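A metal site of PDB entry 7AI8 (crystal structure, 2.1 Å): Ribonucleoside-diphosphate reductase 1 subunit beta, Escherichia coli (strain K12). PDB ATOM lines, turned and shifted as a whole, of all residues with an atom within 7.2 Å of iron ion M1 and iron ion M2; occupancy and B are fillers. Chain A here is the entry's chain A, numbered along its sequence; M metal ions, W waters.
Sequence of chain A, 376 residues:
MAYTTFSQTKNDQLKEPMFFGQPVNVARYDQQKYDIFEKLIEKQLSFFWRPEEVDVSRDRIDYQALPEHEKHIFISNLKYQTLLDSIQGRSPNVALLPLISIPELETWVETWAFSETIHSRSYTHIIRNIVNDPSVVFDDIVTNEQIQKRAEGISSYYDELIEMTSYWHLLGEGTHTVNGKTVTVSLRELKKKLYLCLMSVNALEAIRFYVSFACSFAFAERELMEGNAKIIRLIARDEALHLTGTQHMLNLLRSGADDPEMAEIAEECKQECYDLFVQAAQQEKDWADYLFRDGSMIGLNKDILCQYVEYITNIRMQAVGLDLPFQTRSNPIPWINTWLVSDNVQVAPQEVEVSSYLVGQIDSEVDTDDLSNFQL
The side-chain hydroxyl of Ser 120 is in hydrogen-bond range of the backbone carbonyl oxygen of Glu 116 (3.4 Å). The side-chain carboxylate (OE2) of Glu 205 sits close to the indole nitrogen (NE1) of Trp 112, 2.9 Å away. NE2 of His 242 is in hydrogen-bond range of OG of Ser 115 (2.8 Å). OE2 of Glu 205 sits close to NE2 of Gln 88, at 2.9 Å. The backbone carbonyl oxygen (O) of Asp 85 sits at hydrogen-bond distance from the side-chain hydroxyl (OG) of Ser 120, at 3.1 Å. NE2 of His 242 lies close to O of Asp 238 (3.5 Å). A ring nitrogen (NE2) of His 119 is in hydrogen-bond range of the side-chain carboxylate (OD2) of Asp 238 (2.7 Å). The side-chain carboxylate (OE2) of Glu 116 lies close to the indole nitrogen (NE1) of Trp 112 (3.1 Å).
Four residues have an atom within 4 Å of iron ion M1: Glu 116, Glu 205, Glu 239 and His 242.
Four residues have an atom within 4 Å of iron ion M2: Asp 85, Glu 116, His 119 and Glu 239.
Iron ion M1 is bound by OE2 of Glu 205 (2.0 Å), water W3 (2.0 Å), water W1 (2.1 Å), OE1 of Glu 239 (2.2 Å), ND1 of His 242 (2.3 Å) and OE2 of Glu 116 (2.3 Å). Iron ion M1 has six donor atoms within binding distance.
Iron ion M2 is bound by water W1 (1.9 Å), OD2 of Asp 85 (2.0 Å), OE1 of Glu 116 (2.2 Å), ND1 of His 119 (2.2 Å) and water W2 (2.4 Å). Slightly farther from iron ion M2 lies the side-chain carboxylate (OD1) of Asp 85 (2.8 Å).
Water W3 bridges the side-chain carboxylate (OD1) of Asp 85 (2.8 Å) and the side-chain carboxylate (OE2) of Glu 239 (2.8 Å).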
ATOM      1  N   GLN A  81       1.697 -14.803  17.048  1.00  0.00           N
ATOM      2  CA  GLN A  81       2.501 -15.566  16.095  1.00  0.00           C
ATOM      3  C   GLN A  81       2.479 -14.920  14.721  1.00  0.00           C
ATOM      4  O   GLN A  81       3.527 -14.834  14.055  1.00  0.00           O
ATOM      5  CB  GLN A  81       1.974 -17.006  16.014  1.00  0.00           C
ATOM      6  CG  GLN A  81       2.205 -17.807  17.325  1.00  0.00           C
ATOM      7  CD  GLN A  81       1.513 -19.170  17.355  1.00  0.00           C
ATOM      8  OE1 GLN A  81       0.402 -19.315  16.868  1.00  0.00           O
ATOM      9  NE2 GLN A  81       2.162 -20.154  17.960  1.00  0.00           N
ATOM     10  N   LEU A  84       4.665 -11.939  14.620  1.00  0.00           N
ATOM     11  CA  LEU A  84       6.090 -12.244  14.657  1.00  0.00           C
ATOM     12  C   LEU A  84       6.588 -12.775  13.314  1.00  0.00           C
ATOM     13  O   LEU A  84       7.677 -12.396  12.854  1.00  0.00           O
ATOM     14  CB  LEU A  84       6.404 -13.241  15.772  1.00  0.00           C
ATOM     15  CG  LEU A  84       6.283 -12.780  17.234  1.00  0.00           C
ATOM     16  CD1 LEU A  84       6.608 -13.924  18.254  1.00  0.00           C
ATOM     17  CD2 LEU A  84       7.134 -11.549  17.503  1.00  0.00           C
ATOM     18  N   ASP A  85       5.817 -13.645  12.667  1.00  0.00           N
ATOM     19  CA  ASP A  85       6.280 -14.159  11.383  1.00  0.00           C
ATOM     20  C   ASP A  85       5.919 -13.243  10.210  1.00  0.00           C
ATOM     21  O   ASP A  85       6.452 -13.441   9.112  1.00  0.00           O
ATOM     22  CB  ASP A  85       5.800 -15.610  11.170  1.00  0.00           C
ATOM     23  CG  ASP A  85       6.782 -16.624  11.766  1.00  0.00           C
ATOM     24  OD1 ASP A  85       7.857 -16.195  12.228  1.00  0.00           O
ATOM     25  OD2 ASP A  85       6.502 -17.849  11.795  1.00  0.00           O
ATOM     26  N   GLN A  88       9.259 -11.803  10.446  1.00  0.00           N
ATOM     27  CA  GLN A  88      10.295 -12.751  10.053  1.00  0.00           C
ATOM     28  C   GLN A  88      10.205 -13.135   8.573  1.00  0.00           C
ATOM     29  O   GLN A  88      11.213 -13.550   8.001  1.00  0.00           O
ATOM     30  CB  GLN A  88      10.205 -14.003  10.932  1.00  0.00           C
ATOM     31  CG  GLN A  88      10.725 -13.773  12.338  1.00  0.00           C
ATOM     32  CD  GLN A  88      12.219 -13.532  12.372  1.00  0.00           C
ATOM     33  OE1 GLN A  88      12.672 -12.397  12.471  1.00  0.00           O
ATOM     34  NE2 GLN A  88      12.994 -14.612  12.251  1.00  0.00           N
ATOM     35  N   GLY A  89       9.039 -12.990   7.944  1.00  0.00           N
ATOM     36  CA  GLY A  89       8.948 -13.313   6.529  1.00  0.00           C
ATOM     37  C   GLY A  89       9.805 -12.394   5.686  1.00  0.00           C
ATOM     38  O   GLY A  89      10.519 -12.860   4.798  1.00  0.00           O
ATOM     39  N   TRP A 112      15.451 -19.344   4.778  1.00  0.00           N
ATOM     40  CA  TRP A 112      14.843 -19.064   6.068  1.00  0.00           C
ATOM     41  C   TRP A 112      13.633 -18.154   5.912  1.00  0.00           C
ATOM     42  O   TRP A 112      12.522 -18.495   6.348  1.00  0.00           O
ATOM     43  CB  TRP A 112      15.919 -18.458   6.956  1.00  0.00           C
ATOM     44  CG  TRP A 112      15.523 -17.909   8.285  1.00  0.00           C
ATOM     45  CD1 TRP A 112      14.395 -18.185   9.006  1.00  0.00           C
ATOM     46  CD2 TRP A 112      16.286 -16.970   9.062  1.00  0.00           C
ATOM     47  NE1 TRP A 112      14.412 -17.463  10.181  1.00  0.00           N
ATOM     48  CE2 TRP A 112      15.559 -16.719  10.243  1.00  0.00           C
ATOM     49  CE3 TRP A 112      17.522 -16.336   8.869  1.00  0.00           C
ATOM     50  CZ2 TRP A 112      16.025 -15.840  11.229  1.00  0.00           C
ATOM     51  CZ3 TRP A 112      17.987 -15.457   9.855  1.00  0.00           C
ATOM     52  CH2 TRP A 112      17.236 -15.225  11.019  1.00  0.00           C
ATOM     53  N   SER A 115      10.706 -19.873   4.230  1.00  0.00           N
ATOM     54  CA  SER A 115      10.006 -20.789   5.121  1.00  0.00           C
ATOM     55  C   SER A 115       9.102 -20.020   6.081  1.00  0.00           C
ATOM     56  O   SER A 115       8.055 -20.530   6.503  1.00  0.00           O
ATOM     57  CB  SER A 115      11.015 -21.653   5.876  1.00  0.00           C
ATOM     58  OG  SER A 115      11.595 -20.945   6.960  1.00  0.00           O
ATOM     59  N   GLU A 116       9.466 -18.775   6.411  1.00  0.00           N
ATOM     60  CA  GLU A 116       8.591 -17.939   7.224  1.00  0.00           C
ATOM     61  C   GLU A 116       7.325 -17.548   6.476  1.00  0.00           C
ATOM     62  O   GLU A 116       6.256 -17.446   7.091  1.00  0.00           O
ATOM     63  CB  GLU A 116       9.332 -16.671   7.678  1.00  0.00           C
ATOM     64  CG  GLU A 116      10.614 -16.920   8.426  1.00  0.00           C
ATOM     65  CD  GLU A 116      10.386 -17.409   9.872  1.00  0.00           C
ATOM     66  OE1 GLU A 116       9.284 -17.878  10.219  1.00  0.00           O
ATOM     67  OE2 GLU A 116      11.329 -17.311  10.667  1.00  0.00           O
ATOM     68  N   THR A 117       7.419 -17.303   5.156  1.00  0.00           N
ATOM     69  CA  THR A 117       6.196 -16.956   4.453  1.00  0.00           C
ATOM     70  C   THR A 117       5.216 -18.125   4.469  1.00  0.00           C
ATOM     71  O   THR A 117       4.005 -17.904   4.530  1.00  0.00           O
ATOM     72  CB  THR A 117       6.455 -16.461   3.004  1.00  0.00           C
ATOM     73  OG1 THR A 117       6.881 -17.532   2.147  1.00  0.00           O
ATOM     74  CG2 THR A 117       7.477 -15.303   2.974  1.00  0.00           C
ATOM     75  N   ILE A 118       5.735 -19.361   4.484  1.00  0.00           N
ATOM     76  CA  ILE A 118       4.843 -20.506   4.613  1.00  0.00           C
ATOM     77  C   ILE A 118       4.159 -20.486   5.971  1.00  0.00           C
ATOM     78  O   ILE A 118       2.960 -20.785   6.081  1.00  0.00           O
ATOM     79  CB  ILE A 118       5.618 -21.834   4.407  1.00  0.00           C
ATOM     80  CG1 ILE A 118       6.343 -21.863   3.059  1.00  0.00           C
ATOM     81  CG2 ILE A 118       4.659 -23.027   4.557  1.00  0.00           C
ATOM     82  CD1 ILE A 118       5.420 -21.808   1.821  1.00  0.00           C
ATOM     83  N   HIS A 119       4.894 -20.132   7.022  1.00  0.00           N
ATOM     84  CA  HIS A 119       4.279 -19.990   8.334  1.00  0.00           C
ATOM     85  C   HIS A 119       3.183 -18.937   8.299  1.00  0.00           C
ATOM     86  O   HIS A 119       2.052 -19.182   8.728  1.00  0.00           O
ATOM     87  CB  HIS A 119       5.345 -19.664   9.400  1.00  0.00           C
ATOM     88  CG  HIS A 119       6.389 -20.737   9.561  1.00  0.00           C
ATOM     89  ND1 HIS A 119       7.449 -20.618  10.429  1.00  0.00           N
ATOM     90  CD2 HIS A 119       6.524 -21.937   8.958  1.00  0.00           C
ATOM     91  CE1 HIS A 119       8.202 -21.706  10.353  1.00  0.00           C
ATOM     92  NE2 HIS A 119       7.654 -22.527   9.474  1.00  0.00           N
ATOM     93  N   SER A 120       3.498 -17.749   7.762  1.00  0.00           N
ATOM     94  CA  SER A 120       2.483 -16.710   7.646  1.00  0.00           C
ATOM     95  C   SER A 120       1.255 -17.205   6.871  1.00  0.00           C
ATOM     96  O   SER A 120       0.106 -16.959   7.268  1.00  0.00           O
ATOM     97  CB  SER A 120       3.065 -15.455   6.989  1.00  0.00           C
ATOM     98  OG  SER A 120       4.116 -14.912   7.777  1.00  0.00           O
ATOM     99  N   TYR A 123      -0.814 -19.436   9.108  1.00  0.00           N
ATOM    100  CA  TYR A 123      -1.650 -18.711  10.066  1.00  0.00           C
ATOM    101  C   TYR A 123      -2.920 -18.198   9.391  1.00  0.00           C
ATOM    102  O   TYR A 123      -4.000 -18.223   9.998  1.00  0.00           O
ATOM    103  CB  TYR A 123      -0.858 -17.553  10.694  1.00  0.00           C
ATOM    104  CG  TYR A 123       0.339 -18.016  11.469  1.00  0.00           C
ATOM    105  CD1 TYR A 123       0.230 -19.068  12.383  1.00  0.00           C
ATOM    106  CD2 TYR A 123       1.580 -17.427  11.284  1.00  0.00           C
ATOM    107  CE1 TYR A 123       1.313 -19.502  13.098  1.00  0.00           C
ATOM    108  CE2 TYR A 123       2.678 -17.870  12.000  1.00  0.00           C
ATOM    109  CZ  TYR A 123       2.541 -18.914  12.907  1.00  0.00           C
ATOM    110  OH  TYR A 123       3.611 -19.355  13.639  1.00  0.00           O
ATOM    111  N   LEU A 204      13.737 -13.939  19.654  1.00  0.00           N
ATOM    112  CA  LEU A 204      12.416 -14.014  19.017  1.00  0.00           C
ATOM    113  C   LEU A 204      12.041 -15.460  18.739  1.00  0.00           C
ATOM    114  O   LEU A 204      11.006 -15.959  19.193  1.00  0.00           O
ATOM    115  CB  LEU A 204      12.401 -13.184  17.730  1.00  0.00           C
ATOM    116  CG  LEU A 204      11.128 -12.944  16.893  1.00  0.00           C
ATOM    117  CD1 LEU A 204      11.409 -11.918  15.788  1.00  0.00           C
ATOM    118  CD2 LEU A 204      10.542 -14.211  16.253  1.00  0.00           C
ATOM    119  N   GLU A 205      12.885 -16.157  17.971  1.00  0.00           N
ATOM    120  CA  GLU A 205      12.571 -17.491  17.495  1.00  0.00           C
ATOM    121  C   GLU A 205      12.779 -18.566  18.550  1.00  0.00           C
ATOM    122  O   GLU A 205      12.043 -19.547  18.576  1.00  0.00           O
ATOM    123  CB  GLU A 205      13.410 -17.801  16.249  1.00  0.00           C
ATOM    124  CG  GLU A 205      12.997 -16.929  15.032  1.00  0.00           C
ATOM    125  CD  GLU A 205      13.657 -17.353  13.717  1.00  0.00           C
ATOM    126  OE1 GLU A 205      14.900 -17.493  13.677  1.00  0.00           O
ATOM    127  OE2 GLU A 205      12.927 -17.522  12.719  1.00  0.00           O
ATOM    128  N   PHE A 209       8.662 -17.436  20.349  1.00  0.00           N
ATOM    129  CA  PHE A 209       7.804 -18.394  19.651  1.00  0.00           C
ATOM    130  C   PHE A 209       7.615 -19.669  20.470  1.00  0.00           C
ATOM    131  O   PHE A 209       6.583 -20.338  20.359  1.00  0.00           O
ATOM    132  CB  PHE A 209       8.361 -18.755  18.270  1.00  0.00           C
ATOM    133  CG  PHE A 209       7.622 -18.098  17.148  1.00  0.00           C
ATOM    134  CD1 PHE A 209       8.193 -17.049  16.435  1.00  0.00           C
ATOM    135  CD2 PHE A 209       6.334 -18.510  16.804  1.00  0.00           C
ATOM    136  CE1 PHE A 209       7.500 -16.427  15.395  1.00  0.00           C
ATOM    137  CE2 PHE A 209       5.638 -17.902  15.773  1.00  0.00           C
ATOM    138  CZ  PHE A 209       6.209 -16.853  15.060  1.00  0.00           C
ATOM    139  N   PHE A 213       4.245 -21.636  21.261  1.00  0.00           N
ATOM    140  CA  PHE A 213       4.047 -23.075  21.055  1.00  0.00           C
ATOM    141  C   PHE A 213       3.433 -23.746  22.276  1.00  0.00           C
ATOM    142  O   PHE A 213       2.564 -24.623  22.145  1.00  0.00           O
ATOM    143  CB  PHE A 213       5.378 -23.748  20.716  1.00  0.00           C
ATOM    144  CG  PHE A 213       6.033 -23.259  19.419  1.00  0.00           C
ATOM    145  CD1 PHE A 213       5.296 -22.622  18.442  1.00  0.00           C
ATOM    146  CD2 PHE A 213       7.404 -23.446  19.203  1.00  0.00           C
ATOM    147  CE1 PHE A 213       5.897 -22.169  17.255  1.00  0.00           C
ATOM    148  CE2 PHE A 213       8.015 -23.006  18.055  1.00  0.00           C
ATOM    149  CZ  PHE A 213       7.260 -22.367  17.065  1.00  0.00           C
ATOM    150  N   ILE A 235       5.663 -25.942  12.194  1.00  0.00           N
ATOM    151  CA  ILE A 235       6.324 -24.651  12.381  1.00  0.00           C
ATOM    152  C   ILE A 235       7.470 -24.776  13.388  1.00  0.00           C
ATOM    153  O   ILE A 235       8.589 -24.287  13.168  1.00  0.00           O
ATOM    154  CB  ILE A 235       5.297 -23.589  12.816  1.00  0.00           C
ATOM    155  CG1 ILE A 235       4.331 -23.268  11.655  1.00  0.00           C
ATOM    156  CG2 ILE A 235       5.981 -22.324  13.346  1.00  0.00           C
ATOM    157  CD1 ILE A 235       3.130 -22.364  12.053  1.00  0.00           C
ATOM    158  N   ALA A 236       7.213 -25.463  14.511  1.00  0.00           N
ATOM    159  CA  ALA A 236       8.237 -25.592  15.547  1.00  0.00           C
ATOM    160  C   ALA A 236       9.457 -26.336  15.012  1.00  0.00           C
ATOM    161  O   ALA A 236      10.592 -26.002  15.343  1.00  0.00           O
ATOM    162  CB  ALA A 236       7.671 -26.293  16.781  1.00  0.00           C
ATOM    163  N   ASP A 238      10.551 -26.248  11.963  1.00  0.00           N
ATOM    164  CA  ASP A 238      11.299 -25.239  11.215  1.00  0.00           C
ATOM    165  C   ASP A 238      11.989 -24.270  12.180  1.00  0.00           C
ATOM    166  O   ASP A 238      13.151 -23.884  11.964  1.00  0.00           O
ATOM    167  CB  ASP A 238      10.370 -24.433  10.296  1.00  0.00           C
ATOM    168  CG  ASP A 238       9.752 -25.270   9.169  1.00  0.00           C
ATOM    169  OD1 ASP A 238      10.308 -26.320   8.775  1.00  0.00           O
ATOM    170  OD2 ASP A 238       8.694 -24.843   8.660  1.00  0.00           O
ATOM    171  N   GLU A 239      11.275 -23.848  13.217  1.00  0.00           N
ATOM    172  CA  GLU A 239      11.820 -22.903  14.169  1.00  0.00           C
ATOM    173  C   GLU A 239      13.122 -23.407  14.772  1.00  0.00           C
ATOM    174  O   GLU A 239      14.055 -22.618  15.018  1.00  0.00           O
ATOM    175  CB  GLU A 239      10.795 -22.615  15.261  1.00  0.00           C
ATOM    176  CG  GLU A 239      11.080 -21.351  16.012  1.00  0.00           C
ATOM    177  CD  GLU A 239      10.917 -20.130  15.128  1.00  0.00           C
ATOM    178  OE1 GLU A 239      11.827 -19.851  14.324  1.00  0.00           O
ATOM    179  OE2 GLU A 239       9.859 -19.458  15.241  1.00  0.00           O
ATOM    180  N   ALA A 240      13.228 -24.721  15.004  1.00  0.00           N
ATOM    181  CA  ALA A 240      14.457 -25.254  15.601  1.00  0.00           C
ATOM    182  C   ALA A 240      15.645 -25.043  14.666  1.00  0.00           C
ATOM    183  O   ALA A 240      16.762 -24.751  15.135  1.00  0.00           O
ATOM    184  CB  ALA A 240      14.298 -26.736  15.969  1.00  0.00           C
ATOM    185  N   LEU A 241      15.415 -25.162  13.349  1.00  0.00           N
ATOM    186  CA  LEU A 241      16.442 -24.823  12.361  1.00  0.00           C
ATOM    187  C   LEU A 241      16.771 -23.333  12.385  1.00  0.00           C
ATOM    188  O   LEU A 241      17.942 -22.940  12.272  1.00  0.00           O
ATOM    189  CB  LEU A 241      15.976 -25.215  10.948  1.00  0.00           C
ATOM    190  CG  LEU A 241      15.641 -26.681  10.619  1.00  0.00           C
ATOM    191  CD1 LEU A 241      15.299 -26.794   9.130  1.00  0.00           C
ATOM    192  CD2 LEU A 241      16.799 -27.623  10.992  1.00  0.00           C
ATOM    193  N   HIS A 242      15.746 -22.487  12.532  1.00  0.00           N
ATOM    194  CA  HIS A 242      15.947 -21.054  12.432  1.00  0.00           C
ATOM    195  C   HIS A 242      16.811 -20.560  13.584  1.00  0.00           C
ATOM    196  O   HIS A 242      17.799 -19.844  13.371  1.00  0.00           O
ATOM    197  CB  HIS A 242      14.608 -20.332  12.427  1.00  0.00           C
ATOM    198  CG  HIS A 242      13.730 -20.699  11.273  1.00  0.00           C
ATOM    199  ND1 HIS A 242      12.436 -20.255  11.162  1.00  0.00           N
ATOM    200  CD2 HIS A 242      13.968 -21.473  10.182  1.00  0.00           C
ATOM    201  CE1 HIS A 242      11.911 -20.730  10.047  1.00  0.00           C
ATOM    202  NE2 HIS A 242      12.811 -21.489   9.442  1.00  0.00           N
ATOM    203  N   LEU A 243      16.478 -20.975  14.816  1.00  0.00           N
ATOM    204  CA  LEU A 243      17.273 -20.547  15.950  1.00  0.00           C
ATOM    205  C   LEU A 243      18.673 -21.158  15.909  1.00  0.00           C
ATOM    206  O   LEU A 243      19.622 -20.546  16.410  1.00  0.00           O
ATOM    207  CB  LEU A 243      16.546 -20.879  17.262  1.00  0.00           C
ATOM    208  CG  LEU A 243      16.354 -22.357  17.636  1.00  0.00           C
ATOM    209  CD1 LEU A 243      17.481 -22.836  18.549  1.00  0.00           C
ATOM    210  CD2 LEU A 243      14.999 -22.556  18.302  1.00  0.00           C
HETATM  211 FE    FE M   1      11.340 -18.732  12.459  1.00  0.00          FE
HETATM  212 FE    FE M   2       8.115 -18.946  11.719  1.00  0.00          FE
HETATM  213  O   HOH W   1       9.667 -19.908  12.078  1.00  0.00           O
HETATM  214  O   HOH W   2       7.324 -19.563  13.880  1.00  0.00           O
HETATM  215  O   HOH W   3      10.039 -17.457  13.334  1.00  0.00           O
